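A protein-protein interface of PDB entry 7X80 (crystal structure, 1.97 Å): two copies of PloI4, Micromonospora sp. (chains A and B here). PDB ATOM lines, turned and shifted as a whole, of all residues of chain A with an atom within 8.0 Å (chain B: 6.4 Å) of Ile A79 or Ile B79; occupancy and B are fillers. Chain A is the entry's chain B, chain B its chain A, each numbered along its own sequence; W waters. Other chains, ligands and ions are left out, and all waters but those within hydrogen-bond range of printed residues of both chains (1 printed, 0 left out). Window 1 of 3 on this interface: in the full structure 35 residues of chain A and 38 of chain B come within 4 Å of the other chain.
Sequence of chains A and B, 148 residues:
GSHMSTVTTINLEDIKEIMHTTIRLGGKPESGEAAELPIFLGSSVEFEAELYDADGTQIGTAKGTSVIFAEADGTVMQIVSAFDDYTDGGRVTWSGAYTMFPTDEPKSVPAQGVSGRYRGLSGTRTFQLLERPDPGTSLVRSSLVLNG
Water W1 lies within hydrogen-bond range of O of Ala A82 (2.8 Å), OG of Ser B95 (2.9 Å), O of Trp A94 (3.2 Å) and OG of Ser A81 (3.3 Å).
Of the 26 printed residues of chain A, 9 touch a printed residue of chain B. Hydrophobic or aromatic side chains of chain A that line the printed part of chain B: Val A67, Phe A69 and Ile A79. Of the 14 printed residues of chain B, 8 touch a printed residue of chain A. Among the printed residues, no Asp or Glu carboxylate lies within 4 Å of a Lys or Arg side-chain nitrogen of the other chain.
The side-chain hydroxyl of Ser B81 lies within hydrogen-bond range of the side-chain hydroxyl of Ser A95 (2.8 Å). The backbone NH of Gly B96 sits at hydrogen-bond distance from the side-chain hydroxyl of Ser A81 (3.4 Å). The side-chain hydroxyl (OG) of Ser B95 sits at hydrogen-bond distance from the side-chain hydroxyl (OG) of Ser A81, at 3.1 Å. OG of Ser A95 lies close to OG of Ser B95 (3.3 Å). The side-chain hydroxyl (OG) of Ser B81 lies within hydrogen-bond range of the backbone NH (N) of Gly A96, 3.4 Å away.
The backbone NH (N) of Val A80 sits at hydrogen-bond distance from the backbone carbonyl oxygen (O) of Gly A96. The backbone NH of Met A77 lies within hydrogen-bond range of the backbone carbonyl oxygen of Phe A69 (2.7 Å). The backbone carbonyl oxygen (O) of Val A80 sits at hydrogen-bond distance from the side-chain hydroxyl (OG) of Ser A95, 2.8 Å away. The backbone carbonyl oxygen of Ser A43 sits at hydrogen-bond distance from the backbone NH of Ile A68 (2.9 Å). O of Val B67 sits at hydrogen-bond distance from N of Ile B79, at 2.9 Å. The backbone carbonyl oxygen of Ile A79 lies within hydrogen-bond range of the backbone NH of Val A67.
Val A67 touches Ile B68, and with the chains exchanged Ile A68 touches Val B67. Phe A69 touches Thr B65, but with the chains exchanged Thr A65 does not touch Phe B69 (4.1 Å). Ile A79 touches Ser B81, and with the chains exchanged Ser A81 touches Ile B79. Ser A81 touches Gly B96, and with the chains exchanged Gly A96 touches Ser B81. Positions printed for both chains: 65, 66, 67, 68, 69, 77, 78, 79, 80, 81, 95, 96, 97 and 98.
Of the printed residues of chain B, Ser A44 touches Phe B69. Printed residues of chain B within 4 Å of Thr A65: Ile B79 (3.4 Å). Of chain B, only Thr B65, Val B67, Ile B79 and Ser B81 come within 4 Å of Ile A79. Trp A94 touches none of the printed residues of chain B. Of the printed residues of chain B, Gly A96 touches Ser B81 (3.4 Å). Met A100 touches none of the printed residues of chain B. Of chain A, only Thr A65, Val A67, Ile A79 and Ser A81 come within 4 Å of Ile B79. The nearest residue of chain B that does not touch Ile A79 is Val B80 (4.1 Å).
CB of Ser A44 touches CD2 of Phe B69, at 3.8 Å. Ile B79 touches Thr A65 (CD1 to O, 3.4 Å). CG1 of Val A67 touches O of Ile B68 (3.9 Å). Val A67 touches Phe B69. CG2 of Val A67 touches CG2 of Ile B79, at 3.6 Å. Ile A79 touches Thr B65 (CD1 to O, 3.4 Å). CG2 of Ile A79 touches CG2 of Val B67, at 3.6 Å. Ile A79 touches Ile B79. CD1 of Ile A79 touches N of Ser B81 (3.6 Å). Ser A81 touches Ile B79.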
ATOM      1  N   SER A  43      15.959 -15.092  -5.741  1.00  0.00           N
ATOM      2  CA  SER A  43      17.310 -15.629  -5.695  1.00  0.00           C
ATOM      3  C   SER A  43      18.308 -14.483  -5.705  1.00  0.00           C
ATOM      4  O   SER A  43      18.155 -13.514  -6.459  1.00  0.00           O
ATOM      5  CB  SER A  43      17.552 -16.568  -6.876  1.00  0.00           C
ATOM      6  OG  SER A  43      16.515 -17.528  -6.962  1.00  0.00           O
ATOM      7  N   SER A  44      19.302 -14.572  -4.830  1.00  0.00           N
ATOM      8  CA  SER A  44      20.261 -13.492  -4.626  1.00  0.00           C
ATOM      9  C   SER A  44      21.688 -14.032  -4.675  1.00  0.00           C
ATOM     10  O   SER A  44      21.959 -15.209  -4.383  1.00  0.00           O
ATOM     11  CB  SER A  44      20.027 -12.803  -3.278  1.00  0.00           C
ATOM     12  OG  SER A  44      20.059 -13.777  -2.226  1.00  0.00           O
ATOM     13  N   VAL A  45      22.601 -13.137  -5.027  1.00  0.00           N
ATOM     14  CA  VAL A  45      24.033 -13.381  -4.978  1.00  0.00           C
ATOM     15  C   VAL A  45      24.633 -12.245  -4.172  1.00  0.00           C
ATOM     16  O   VAL A  45      24.490 -11.078  -4.547  1.00  0.00           O
ATOM     17  CB  VAL A  45      24.666 -13.432  -6.381  1.00  0.00           C
ATOM     18  CG1 VAL A  45      26.177 -13.661  -6.282  1.00  0.00           C
ATOM     19  CG2 VAL A  45      24.012 -14.501  -7.236  1.00  0.00           C
ATOM     20  N   PHE A  47      28.333 -10.971  -3.131  1.00  0.00           N
ATOM     21  CA  PHE A  47      29.683 -11.268  -3.581  1.00  0.00           C
ATOM     22  C   PHE A  47      30.706 -10.282  -3.037  1.00  0.00           C
ATOM     23  O   PHE A  47      30.399  -9.123  -2.717  1.00  0.00           O
ATOM     24  CB  PHE A  47      29.784 -11.298  -5.110  1.00  0.00           C
ATOM     25  CG  PHE A  47      29.434  -9.986  -5.789  1.00  0.00           C
ATOM     26  CD1 PHE A  47      30.407  -9.025  -6.025  1.00  0.00           C
ATOM     27  CD2 PHE A  47      28.141  -9.745  -6.232  1.00  0.00           C
ATOM     28  CE1 PHE A  47      30.081  -7.828  -6.668  1.00  0.00           C
ATOM     29  CE2 PHE A  47      27.817  -8.558  -6.872  1.00  0.00           C
ATOM     30  CZ  PHE A  47      28.791  -7.610  -7.097  1.00  0.00           C
ATOM     31  N   GLY A  64      29.150  -6.472  -3.632  1.00  0.00           N
ATOM     32  CA  GLY A  64      27.817  -6.111  -4.072  1.00  0.00           C
ATOM     33  C   GLY A  64      26.815  -7.218  -3.836  1.00  0.00           C
ATOM     34  O   GLY A  64      27.117  -8.266  -3.250  1.00  0.00           O
ATOM     35  N   THR A  65      25.600  -6.948  -4.299  1.00  0.00           N
ATOM     36  CA  THR A  65      24.472  -7.861  -4.210  1.00  0.00           C
ATOM     37  C   THR A  65      23.716  -7.807  -5.522  1.00  0.00           C
ATOM     38  O   THR A  65      23.506  -6.724  -6.071  1.00  0.00           O
ATOM     39  CB  THR A  65      23.512  -7.485  -3.074  1.00  0.00           C
ATOM     40  OG1 THR A  65      24.232  -7.360  -1.842  1.00  0.00           O
ATOM     41  CG2 THR A  65      22.416  -8.545  -2.930  1.00  0.00           C
ATOM     42  N   SER A  66      23.294  -8.963  -6.017  1.00  0.00           N
ATOM     43  CA  SER A  66      22.347  -8.997  -7.123  1.00  0.00           C
ATOM     44  C   SER A  66      21.179  -9.913  -6.771  1.00  0.00           C
ATOM     45  O   SER A  66      21.320 -10.835  -5.959  1.00  0.00           O
ATOM     46  CB  SER A  66      23.023  -9.408  -8.444  1.00  0.00           C
ATOM     47  OG  SER A  66      23.447 -10.759  -8.426  1.00  0.00           O
ATOM     48  N   VAL A  67      20.007  -9.615  -7.347  1.00  0.00           N
ATOM     49  CA  VAL A  67      18.763 -10.340  -7.071  1.00  0.00           C
ATOM     50  C   VAL A  67      17.998 -10.533  -8.384  1.00  0.00           C
ATOM     51  O   VAL A  67      17.902  -9.612  -9.204  1.00  0.00           O
ATOM     52  CB  VAL A  67      17.890  -9.593  -6.028  1.00  0.00           C
ATOM     53  CG1 VAL A  67      16.605 -10.402  -5.695  1.00  0.00           C
ATOM     54  CG2 VAL A  67      18.680  -9.298  -4.749  1.00  0.00           C
ATOM     55  N   ILE A  68      17.418 -11.719  -8.569  1.00  0.00           N
ATOM     56  CA  ILE A  68      16.654 -12.031  -9.778  1.00  0.00           C
ATOM     57  C   ILE A  68      15.218 -11.522  -9.648  1.00  0.00           C
ATOM     58  O   ILE A  68      14.595 -11.627  -8.582  1.00  0.00           O
ATOM     59  CB  ILE A  68      16.676 -13.550 -10.053  1.00  0.00           C
ATOM     60  CG1 ILE A  68      18.113 -14.061 -10.297  1.00  0.00           C
ATOM     61  CG2 ILE A  68      15.749 -13.895 -11.210  1.00  0.00           C
ATOM     62  CD1 ILE A  68      18.193 -15.593 -10.501  1.00  0.00           C
ATOM     63  N   PHE A  69      14.685 -10.963 -10.735  1.00  0.00           N
ATOM     64  CA  PHE A  69      13.269 -10.593 -10.813  1.00  0.00           C
ATOM     65  C   PHE A  69      12.845 -10.660 -12.278  1.00  0.00           C
ATOM     66  O   PHE A  69      13.621 -11.075 -13.141  1.00  0.00           O
ATOM     67  CB  PHE A  69      13.008  -9.206 -10.199  1.00  0.00           C
ATOM     68  CG  PHE A  69      13.525  -8.052 -11.031  1.00  0.00           C
ATOM     69  CD1 PHE A  69      14.881  -7.759 -11.081  1.00  0.00           C
ATOM     70  CD2 PHE A  69      12.638  -7.240 -11.739  1.00  0.00           C
ATOM     71  CE1 PHE A  69      15.345  -6.680 -11.832  1.00  0.00           C
ATOM     72  CE2 PHE A  69      13.090  -6.168 -12.493  1.00  0.00           C
ATOM     73  CZ  PHE A  69      14.455  -5.886 -12.546  1.00  0.00           C
ATOM     74  N   VAL A  76      13.417 -12.210 -17.745  1.00  0.00           N
ATOM     75  CA  VAL A  76      14.076 -12.416 -16.463  1.00  0.00           C
ATOM     76  C   VAL A  76      15.257 -11.461 -16.352  1.00  0.00           C
ATOM     77  O   VAL A  76      16.105 -11.386 -17.251  1.00  0.00           O
ATOM     78  CB  VAL A  76      14.509 -13.878 -16.300  1.00  0.00           C
ATOM     79  CG1 VAL A  76      15.144 -14.073 -14.935  1.00  0.00           C
ATOM     80  CG2 VAL A  76      13.302 -14.772 -16.437  1.00  0.00           C
ATOM     81  N   MET A  77      15.307 -10.728 -15.246  1.00  0.00           N
ATOM     82  CA  MET A  77      16.217  -9.622 -15.039  1.00  0.00           C
ATOM     83  C   MET A  77      17.031  -9.917 -13.780  1.00  0.00           C
ATOM     84  O   MET A  77      16.661 -10.761 -12.963  1.00  0.00           O
ATOM     85  CB  MET A  77      15.416  -8.323 -14.853  1.00  0.00           C
ATOM     86  CG  MET A  77      14.691  -7.827 -16.115  1.00  0.00           C
ATOM     87  SD  MET A  77      15.631  -7.497 -17.623  1.00  0.00           S
ATOM     88  CE  MET A  77      16.555  -6.041 -17.126  1.00  0.00           C
ATOM     89  N   GLN A  78      18.151  -9.228 -13.629  1.00  0.00           N
ATOM     90  CA  GLN A  78      18.837  -9.132 -12.351  1.00  0.00           C
ATOM     91  C   GLN A  78      19.039  -7.666 -12.037  1.00  0.00           C
ATOM     92  O   GLN A  78      19.305  -6.867 -12.937  1.00  0.00           O
ATOM     93  CB  GLN A  78      20.181  -9.888 -12.369  1.00  0.00           C
ATOM     94  CG  GLN A  78      19.972 -11.377 -12.666  1.00  0.00           C
ATOM     95  CD  GLN A  78      21.220 -12.237 -12.500  1.00  0.00           C
ATOM     96  OE1 GLN A  78      22.283 -11.757 -12.107  1.00  0.00           O
ATOM     97  NE2 GLN A  78      21.078 -13.533 -12.774  1.00  0.00           N
ATOM     98  N   ILE A  79      18.872  -7.311 -10.771  1.00  0.00           N
ATOM     99  CA  ILE A  79      19.250  -5.996 -10.273  1.00  0.00           C
ATOM    100  C   ILE A  79      20.515  -6.171  -9.447  1.00  0.00           C
ATOM    101  O   ILE A  79      20.646  -7.152  -8.709  1.00  0.00           O
ATOM    102  CB  ILE A  79      18.121  -5.355  -9.452  1.00  0.00           C
ATOM    103  CG1 ILE A  79      18.568  -4.006  -8.885  1.00  0.00           C
ATOM    104  CG2 ILE A  79      17.603  -6.327  -8.345  1.00  0.00           C
ATOM    105  CD1 ILE A  79      17.391  -3.097  -8.501  1.00  0.00           C
ATOM    106  N   VAL A  80      21.461  -5.245  -9.587  1.00  0.00           N
ATOM    107  CA  VAL A  80      22.700  -5.316  -8.820  1.00  0.00           C
ATOM    108  C   VAL A  80      22.960  -3.948  -8.201  1.00  0.00           C
ATOM    109  O   VAL A  80      22.593  -2.917  -8.772  1.00  0.00           O
ATOM    110  CB  VAL A  80      23.888  -5.796  -9.692  1.00  0.00           C
ATOM    111  CG1 VAL A  80      24.170  -4.843 -10.847  1.00  0.00           C
ATOM    112  CG2 VAL A  80      25.182  -5.984  -8.850  1.00  0.00           C
ATOM    113  N   SER A  81      23.523  -3.942  -6.996  1.00  0.00           N
ATOM    114  CA  SER A  81      24.066  -2.731  -6.392  1.00  0.00           C
ATOM    115  C   SER A  81      25.421  -3.096  -5.819  1.00  0.00           C
ATOM    116  O   SER A  81      25.522  -4.034  -5.018  1.00  0.00           O
ATOM    117  CB  SER A  81      23.156  -2.172  -5.291  1.00  0.00           C
ATOM    118  OG  SER A  81      23.775  -1.045  -4.674  1.00  0.00           O
ATOM    119  N   ALA A  82      26.457  -2.370  -6.224  1.00  0.00           N
ATOM    120  CA  ALA A  82      27.818  -2.798  -5.929  1.00  0.00           C
ATOM    121  C   ALA A  82      28.746  -1.594  -5.988  1.00  0.00           C
ATOM    122  O   ALA A  82      28.339  -0.475  -6.316  1.00  0.00           O
ATOM    123  CB  ALA A  82      28.266  -3.897  -6.900  1.00  0.00           C
ATOM    124  N   TRP A  94      28.412   1.105  -8.698  1.00  0.00           N
ATOM    125  CA  TRP A  94      27.711   0.750  -9.925  1.00  0.00           C
ATOM    126  C   TRP A  94      26.446  -0.011  -9.561  1.00  0.00           C
ATOM    127  O   TRP A  94      26.422  -0.764  -8.583  1.00  0.00           O
ATOM    128  CB  TRP A  94      28.592  -0.058 -10.907  1.00  0.00           C
ATOM    129  CG  TRP A  94      29.415  -1.204 -10.325  1.00  0.00           C
ATOM    130  CD1 TRP A  94      30.627  -1.105  -9.700  1.00  0.00           C
ATOM    131  CD2 TRP A  94      29.103  -2.615 -10.376  1.00  0.00           C
ATOM    132  NE1 TRP A  94      31.076  -2.359  -9.329  1.00  0.00           N
ATOM    133  CE2 TRP A  94      30.157  -3.300  -9.725  1.00  0.00           C
ATOM    134  CE3 TRP A  94      28.030  -3.360 -10.894  1.00  0.00           C
ATOM    135  CZ2 TRP A  94      30.183  -4.699  -9.600  1.00  0.00           C
ATOM    136  CZ3 TRP A  94      28.043  -4.764 -10.750  1.00  0.00           C
ATOM    137  CH2 TRP A  94      29.115  -5.412 -10.109  1.00  0.00           C
ATOM    138  N   SER A  95      25.399   0.187 -10.364  1.00  0.00           N
ATOM    139  CA  SER A  95      24.089  -0.354 -10.036  1.00  0.00           C
ATOM    140  C   SER A  95      23.157  -0.215 -11.234  1.00  0.00           C
ATOM    141  O   SER A  95      23.225   0.777 -11.965  1.00  0.00           O
ATOM    142  CB  SER A  95      23.506   0.380  -8.822  1.00  0.00           C
ATOM    143  OG  SER A  95      22.252  -0.127  -8.472  1.00  0.00           O
ATOM    144  N   GLY A  96      22.263  -1.177 -11.382  1.00  0.00           N
ATOM    145  CA  GLY A  96      21.245  -1.135 -12.408  1.00  0.00           C
ATOM    146  C   GLY A  96      20.626  -2.508 -12.553  1.00  0.00           C
ATOM    147  O   GLY A  96      20.985  -3.452 -11.853  1.00  0.00           O
ATOM    148  N   ALA A  97      19.705  -2.606 -13.504  1.00  0.00           N
ATOM    149  CA  ALA A  97      19.145  -3.891 -13.897  1.00  0.00           C
ATOM    150  C   ALA A  97      19.653  -4.290 -15.281  1.00  0.00           C
ATOM    151  O   ALA A  97      19.860  -3.444 -16.154  1.00  0.00           O
ATOM    152  CB  ALA A  97      17.615  -3.855 -13.888  1.00  0.00           C
ATOM    153  N   TYR A  98      19.850  -5.592 -15.477  1.00  0.00           N
ATOM    154  CA  TYR A  98      20.308  -6.134 -16.753  1.00  0.00           C
ATOM    155  C   TYR A  98      19.611  -7.468 -16.992  1.00  0.00           C
ATOM    156  O   TYR A  98      19.146  -8.123 -16.057  1.00  0.00           O
ATOM    157  CB  TYR A  98      21.844  -6.308 -16.789  1.00  0.00           C
ATOM    158  CG  TYR A  98      22.368  -7.160 -15.665  1.00  0.00           C
ATOM    159  CD1 TYR A  98      22.469  -8.533 -15.807  1.00  0.00           C
ATOM    160  CD2 TYR A  98      22.691  -6.600 -14.436  1.00  0.00           C
ATOM    161  CE1 TYR A  98      22.915  -9.323 -14.777  1.00  0.00           C
ATOM    162  CE2 TYR A  98      23.139  -7.385 -13.391  1.00  0.00           C
ATOM    163  CZ  TYR A  98      23.249  -8.746 -13.569  1.00  0.00           C
ATOM    164  OH  TYR A  98      23.690  -9.545 -12.542  1.00  0.00           O
ATOM    165  N   THR A  99      19.542  -7.869 -18.258  1.00  0.00           N
ATOM    166  CA  THR A  99      18.926  -9.145 -18.594  1.00  0.00           C
ATOM    167  C   THR A  99      19.765 -10.303 -18.072  1.00  0.00           C
ATOM    168  O   THR A  99      20.994 -10.301 -18.170  1.00  0.00           O
ATOM    169  CB  THR A  99      18.752  -9.277 -20.104  1.00  0.00           C
ATOM    170  OG1 THR A  99      20.049  -9.311 -20.720  1.00  0.00           O
ATOM    171  CG2 THR A  99      17.961  -8.097 -20.647  1.00  0.00           C
ATOM    172  N   MET A 100      19.094 -11.299 -17.503  1.00  0.00           N
ATOM    173  CA  MET A 100      19.824 -12.466 -17.024  1.00  0.00           C
ATOM    174  C   MET A 100      20.345 -13.307 -18.179  1.00  0.00           C
ATOM    175  O   MET A 100      21.490 -13.772 -18.148  1.00  0.00           O
ATOM    176  CB  MET A 100      18.941 -13.299 -16.104  1.00  0.00           C
ATOM    177  CG  MET A 100      19.660 -14.547 -15.589  1.00  0.00           C
ATOM    178  SD  MET A 100      18.707 -15.368 -14.321  1.00  0.00           S
ATOM    179  CE  MET A 100      19.772 -16.771 -13.925  1.00  0.00           C
ATOM    180  N   VAL A 109      25.942  -1.969 -16.415  1.00  0.00           N
ATOM    181  CA  VAL A 109      25.081  -1.021 -15.712  1.00  0.00           C
ATOM    182  C   VAL A 109      25.870   0.264 -15.502  1.00  0.00           C
ATOM    183  O   VAL A 109      27.106   0.270 -15.598  1.00  0.00           O
ATOM    184  CB  VAL A 109      24.597  -1.577 -14.353  1.00  0.00           C
ATOM    185  CG1 VAL A 109      23.796  -2.874 -14.531  1.00  0.00           C
ATOM    186  CG2 VAL A 109      25.795  -1.758 -13.390  1.00  0.00           C
ATOM    187  N   PHE A 127      30.764  -6.558 -17.036  1.00  0.00           N
ATOM    188  CA  PHE A 127      31.030  -7.842 -16.407  1.00  0.00           C
ATOM    189  C   PHE A 127      30.415  -8.979 -17.198  1.00  0.00           C
ATOM    190  O   PHE A 127      29.271  -8.888 -17.656  1.00  0.00           O
ATOM    191  CB  PHE A 127      30.654  -7.783 -14.913  1.00  0.00           C
ATOM    192  CG  PHE A 127      29.214  -7.452 -14.645  1.00  0.00           C
ATOM    193  CD1 PHE A 127      28.903  -6.103 -14.494  1.00  0.00           C
ATOM    194  CD2 PHE A 127      28.187  -8.369 -14.660  1.00  0.00           C
ATOM    195  CE1 PHE A 127      27.613  -5.675 -14.257  1.00  0.00           C
ATOM    196  CE2 PHE A 127      26.874  -7.948 -14.428  1.00  0.00           C
ATOM    197  CZ  PHE A 127      26.591  -6.591 -14.231  1.00  0.00           C
ATOM    198  N   THR B  65      13.902   0.770  -9.454  1.00  0.00           N
ATOM    199  CA  THR B  65      13.382  -0.578  -9.226  1.00  0.00           C
ATOM    200  C   THR B  65      13.828  -1.104  -7.879  1.00  0.00           C
ATOM    201  O   THR B  65      14.972  -0.897  -7.482  1.00  0.00           O
ATOM    202  CB  THR B  65      13.841  -1.562 -10.312  1.00  0.00           C
ATOM    203  OG1 THR B  65      13.694  -0.976 -11.609  1.00  0.00           O
ATOM    204  CG2 THR B  65      13.172  -2.957 -10.191  1.00  0.00           C
ATOM    205  N   SER B  66      12.917  -1.790  -7.172  1.00  0.00           N
ATOM    206  CA  SER B  66      13.298  -2.489  -5.958  1.00  0.00           C
ATOM    207  C   SER B  66      12.799  -3.925  -6.037  1.00  0.00           C
ATOM    208  O   SER B  66      11.817  -4.230  -6.728  1.00  0.00           O
ATOM    209  CB  SER B  66      12.774  -1.801  -4.684  1.00  0.00           C
ATOM    210  OG  SER B  66      11.367  -1.815  -4.621  1.00  0.00           O
ATOM    211  N   VAL B  67      13.530  -4.818  -5.363  1.00  0.00           N
ATOM    212  CA  VAL B  67      13.235  -6.250  -5.363  1.00  0.00           C
ATOM    213  C   VAL B  67      13.453  -6.799  -3.962  1.00  0.00           C
ATOM    214  O   VAL B  67      14.420  -6.434  -3.289  1.00  0.00           O
ATOM    215  CB  VAL B  67      14.111  -7.038  -6.375  1.00  0.00           C
ATOM    216  CG1 VAL B  67      13.657  -8.506  -6.426  1.00  0.00           C
ATOM    217  CG2 VAL B  67      14.065  -6.411  -7.767  1.00  0.00           C
ATOM    218  N   ILE B  68      12.572  -7.717  -3.535  1.00  0.00           N
ATOM    219  CA  ILE B  68      12.684  -8.336  -2.219  1.00  0.00           C
ATOM    220  C   ILE B  68      13.586  -9.567  -2.300  1.00  0.00           C
ATOM    221  O   ILE B  68      13.532 -10.346  -3.261  1.00  0.00           O
ATOM    222  CB  ILE B  68      11.288  -8.696  -1.670  1.00  0.00           C
ATOM    223  CG1 ILE B  68      10.439  -7.436  -1.502  1.00  0.00           C
ATOM    224  CG2 ILE B  68      11.417  -9.422  -0.345  1.00  0.00           C
ATOM    225  CD1 ILE B  68       9.024  -7.717  -0.963  1.00  0.00           C
ATOM    226  N   PHE B  69      14.433  -9.734  -1.289  1.00  0.00           N
ATOM    227  CA  PHE B  69      15.233 -10.944  -1.121  1.00  0.00           C
ATOM    228  C   PHE B  69      15.416 -11.166   0.375  1.00  0.00           C
ATOM    229  O   PHE B  69      14.790 -10.482   1.189  1.00  0.00           O
ATOM    230  CB  PHE B  69      16.553 -10.827  -1.895  1.00  0.00           C
ATOM    231  CG  PHE B  69      17.553  -9.900  -1.270  1.00  0.00           C
ATOM    232  CD1 PHE B  69      17.416  -8.524  -1.404  1.00  0.00           C
ATOM    233  CD2 PHE B  69      18.665 -10.399  -0.600  1.00  0.00           C
ATOM    234  CE1 PHE B  69      18.347  -7.659  -0.851  1.00  0.00           C
ATOM    235  CE2 PHE B  69      19.607  -9.538  -0.049  1.00  0.00           C
ATOM    236  CZ  PHE B  69      19.443  -8.162  -0.172  1.00  0.00           C
ATOM    237  N   MET B  77      14.919  -8.451   3.102  1.00  0.00           N
ATOM    238  CA  MET B  77      15.537  -7.233   2.586  1.00  0.00           C
ATOM    239  C   MET B  77      14.903  -6.762   1.282  1.00  0.00           C
ATOM    240  O   MET B  77      14.180  -7.496   0.605  1.00  0.00           O
ATOM    241  CB  MET B  77      17.051  -7.408   2.341  1.00  0.00           C
ATOM    242  CG  MET B  77      17.808  -8.245   3.336  1.00  0.00           C
ATOM    243  SD  MET B  77      18.087  -7.212   4.806  1.00  0.00           S
ATOM    244  CE  MET B  77      19.277  -6.027   4.141  1.00  0.00           C
ATOM    245  N   GLN B  78      15.201  -5.506   0.932  1.00  0.00           N
ATOM    246  CA  GLN B  78      14.926  -4.977  -0.393  1.00  0.00           C
ATOM    247  C   GLN B  78      16.233  -4.457  -0.972  1.00  0.00           C
ATOM    248  O   GLN B  78      17.070  -3.931  -0.239  1.00  0.00           O
ATOM    249  CB  GLN B  78      13.868  -3.853  -0.348  1.00  0.00           C
ATOM    250  CG  GLN B  78      12.557  -4.269   0.301  1.00  0.00           C
ATOM    251  CD  GLN B  78      11.410  -3.290   0.056  1.00  0.00           C
ATOM    252  OE1 GLN B  78      11.621  -2.131  -0.298  1.00  0.00           O
ATOM    253  NE2 GLN B  78      10.192  -3.757   0.244  1.00  0.00           N
ATOM    254  N   ILE B  79      16.421  -4.627  -2.271  1.00  0.00           N
ATOM    255  CA  ILE B  79      17.507  -3.969  -2.993  1.00  0.00           C
ATOM    256  C   ILE B  79      16.865  -2.954  -3.924  1.00  0.00           C
ATOM    257  O   ILE B  79      15.825  -3.234  -4.524  1.00  0.00           O
ATOM    258  CB  ILE B  79      18.382  -4.988  -3.755  1.00  0.00           C
ATOM    259  CG1 ILE B  79      19.560  -4.306  -4.487  1.00  0.00           C
ATOM    260  CG2 ILE B  79      17.540  -5.833  -4.707  1.00  0.00           C
ATOM    261  CD1 ILE B  79      20.550  -5.306  -5.074  1.00  0.00           C
ATOM    262  N   VAL B  80      17.440  -1.760  -4.010  1.00  0.00           N
ATOM    263  CA  VAL B  80      16.893  -0.719  -4.871  1.00  0.00           C
ATOM    264  C   VAL B  80      18.029  -0.142  -5.710  1.00  0.00           C
ATOM    265  O   VAL B  80      19.169  -0.055  -5.249  1.00  0.00           O
ATOM    266  CB  VAL B  80      16.173   0.384  -4.051  1.00  0.00           C
ATOM    267  CG1 VAL B  80      17.154   1.108  -3.117  1.00  0.00           C
ATOM    268  CG2 VAL B  80      15.433   1.404  -4.971  1.00  0.00           C
ATOM    269  N   SER B  81      17.732   0.174  -6.970  1.00  0.00           N
ATOM    270  CA  SER B  81      18.627   0.958  -7.825  1.00  0.00           C
ATOM    271  C   SER B  81      17.779   2.075  -8.413  1.00  0.00           C
ATOM    272  O   SER B  81      16.748   1.801  -9.033  1.00  0.00           O
ATOM    273  CB  SER B  81      19.269   0.096  -8.934  1.00  0.00           C
ATOM    274  OG  SER B  81      20.077   0.892  -9.823  1.00  0.00           O
ATOM    275  N   SER B  95      21.397   3.657  -4.524  1.00  0.00           N
ATOM    276  CA  SER B  95      21.159   2.224  -4.600  1.00  0.00           C
ATOM    277  C   SER B  95      21.783   1.538  -3.397  1.00  0.00           C
ATOM    278  O   SER B  95      22.760   2.019  -2.811  1.00  0.00           O
ATOM    279  CB  SER B  95      21.735   1.619  -5.884  1.00  0.00           C
ATOM    280  OG  SER B  95      23.141   1.705  -5.882  1.00  0.00           O
ATOM    281  N   GLY B  96      21.203   0.399  -3.041  1.00  0.00           N
ATOM    282  CA  GLY B  96      21.703  -0.373  -1.927  1.00  0.00           C
ATOM    283  C   GLY B  96      20.643  -1.367  -1.490  1.00  0.00           C
ATOM    284  O   GLY B  96      19.625  -1.558  -2.154  1.00  0.00           O
ATOM    285  N   ALA B  97      20.923  -2.004  -0.366  1.00  0.00           N
ATOM    286  CA  ALA B  97      20.026  -2.979   0.236  1.00  0.00           C
ATOM    287  C   ALA B  97      19.709  -2.528   1.649  1.00  0.00           C
ATOM    288  O   ALA B  97      20.588  -2.030   2.360  1.00  0.00           O
ATOM    289  CB  ALA B  97      20.645  -4.377   0.252  1.00  0.00           C
ATOM    290  N   TYR B  98      18.457  -2.708   2.058  1.00  0.00           N
ATOM    291  CA  TYR B  98      18.009  -2.286   3.376  1.00  0.00           C
ATOM    292  C   TYR B  98      17.034  -3.319   3.930  1.00  0.00           C
ATOM    293  O   TYR B  98      16.434  -4.094   3.180  1.00  0.00           O
ATOM    294  CB  TYR B  98      17.357  -0.903   3.326  1.00  0.00           C
ATOM    295  CG  TYR B  98      16.222  -0.773   2.330  1.00  0.00           C
ATOM    296  CD1 TYR B  98      16.470  -0.408   0.998  1.00  0.00           C
ATOM    297  CD2 TYR B  98      14.898  -0.979   2.732  1.00  0.00           C
ATOM    298  CE1 TYR B  98      15.429  -0.273   0.098  1.00  0.00           C
ATOM    299  CE2 TYR B  98      13.860  -0.838   1.851  1.00  0.00           C
ATOM    300  CZ  TYR B  98      14.125  -0.492   0.538  1.00  0.00           C
ATOM    301  OH  TYR B  98      13.075  -0.378  -0.322  1.00  0.00           O
HETATM  302  O   HOH W   1      25.992   1.092  -5.971  1.00  0.00           O
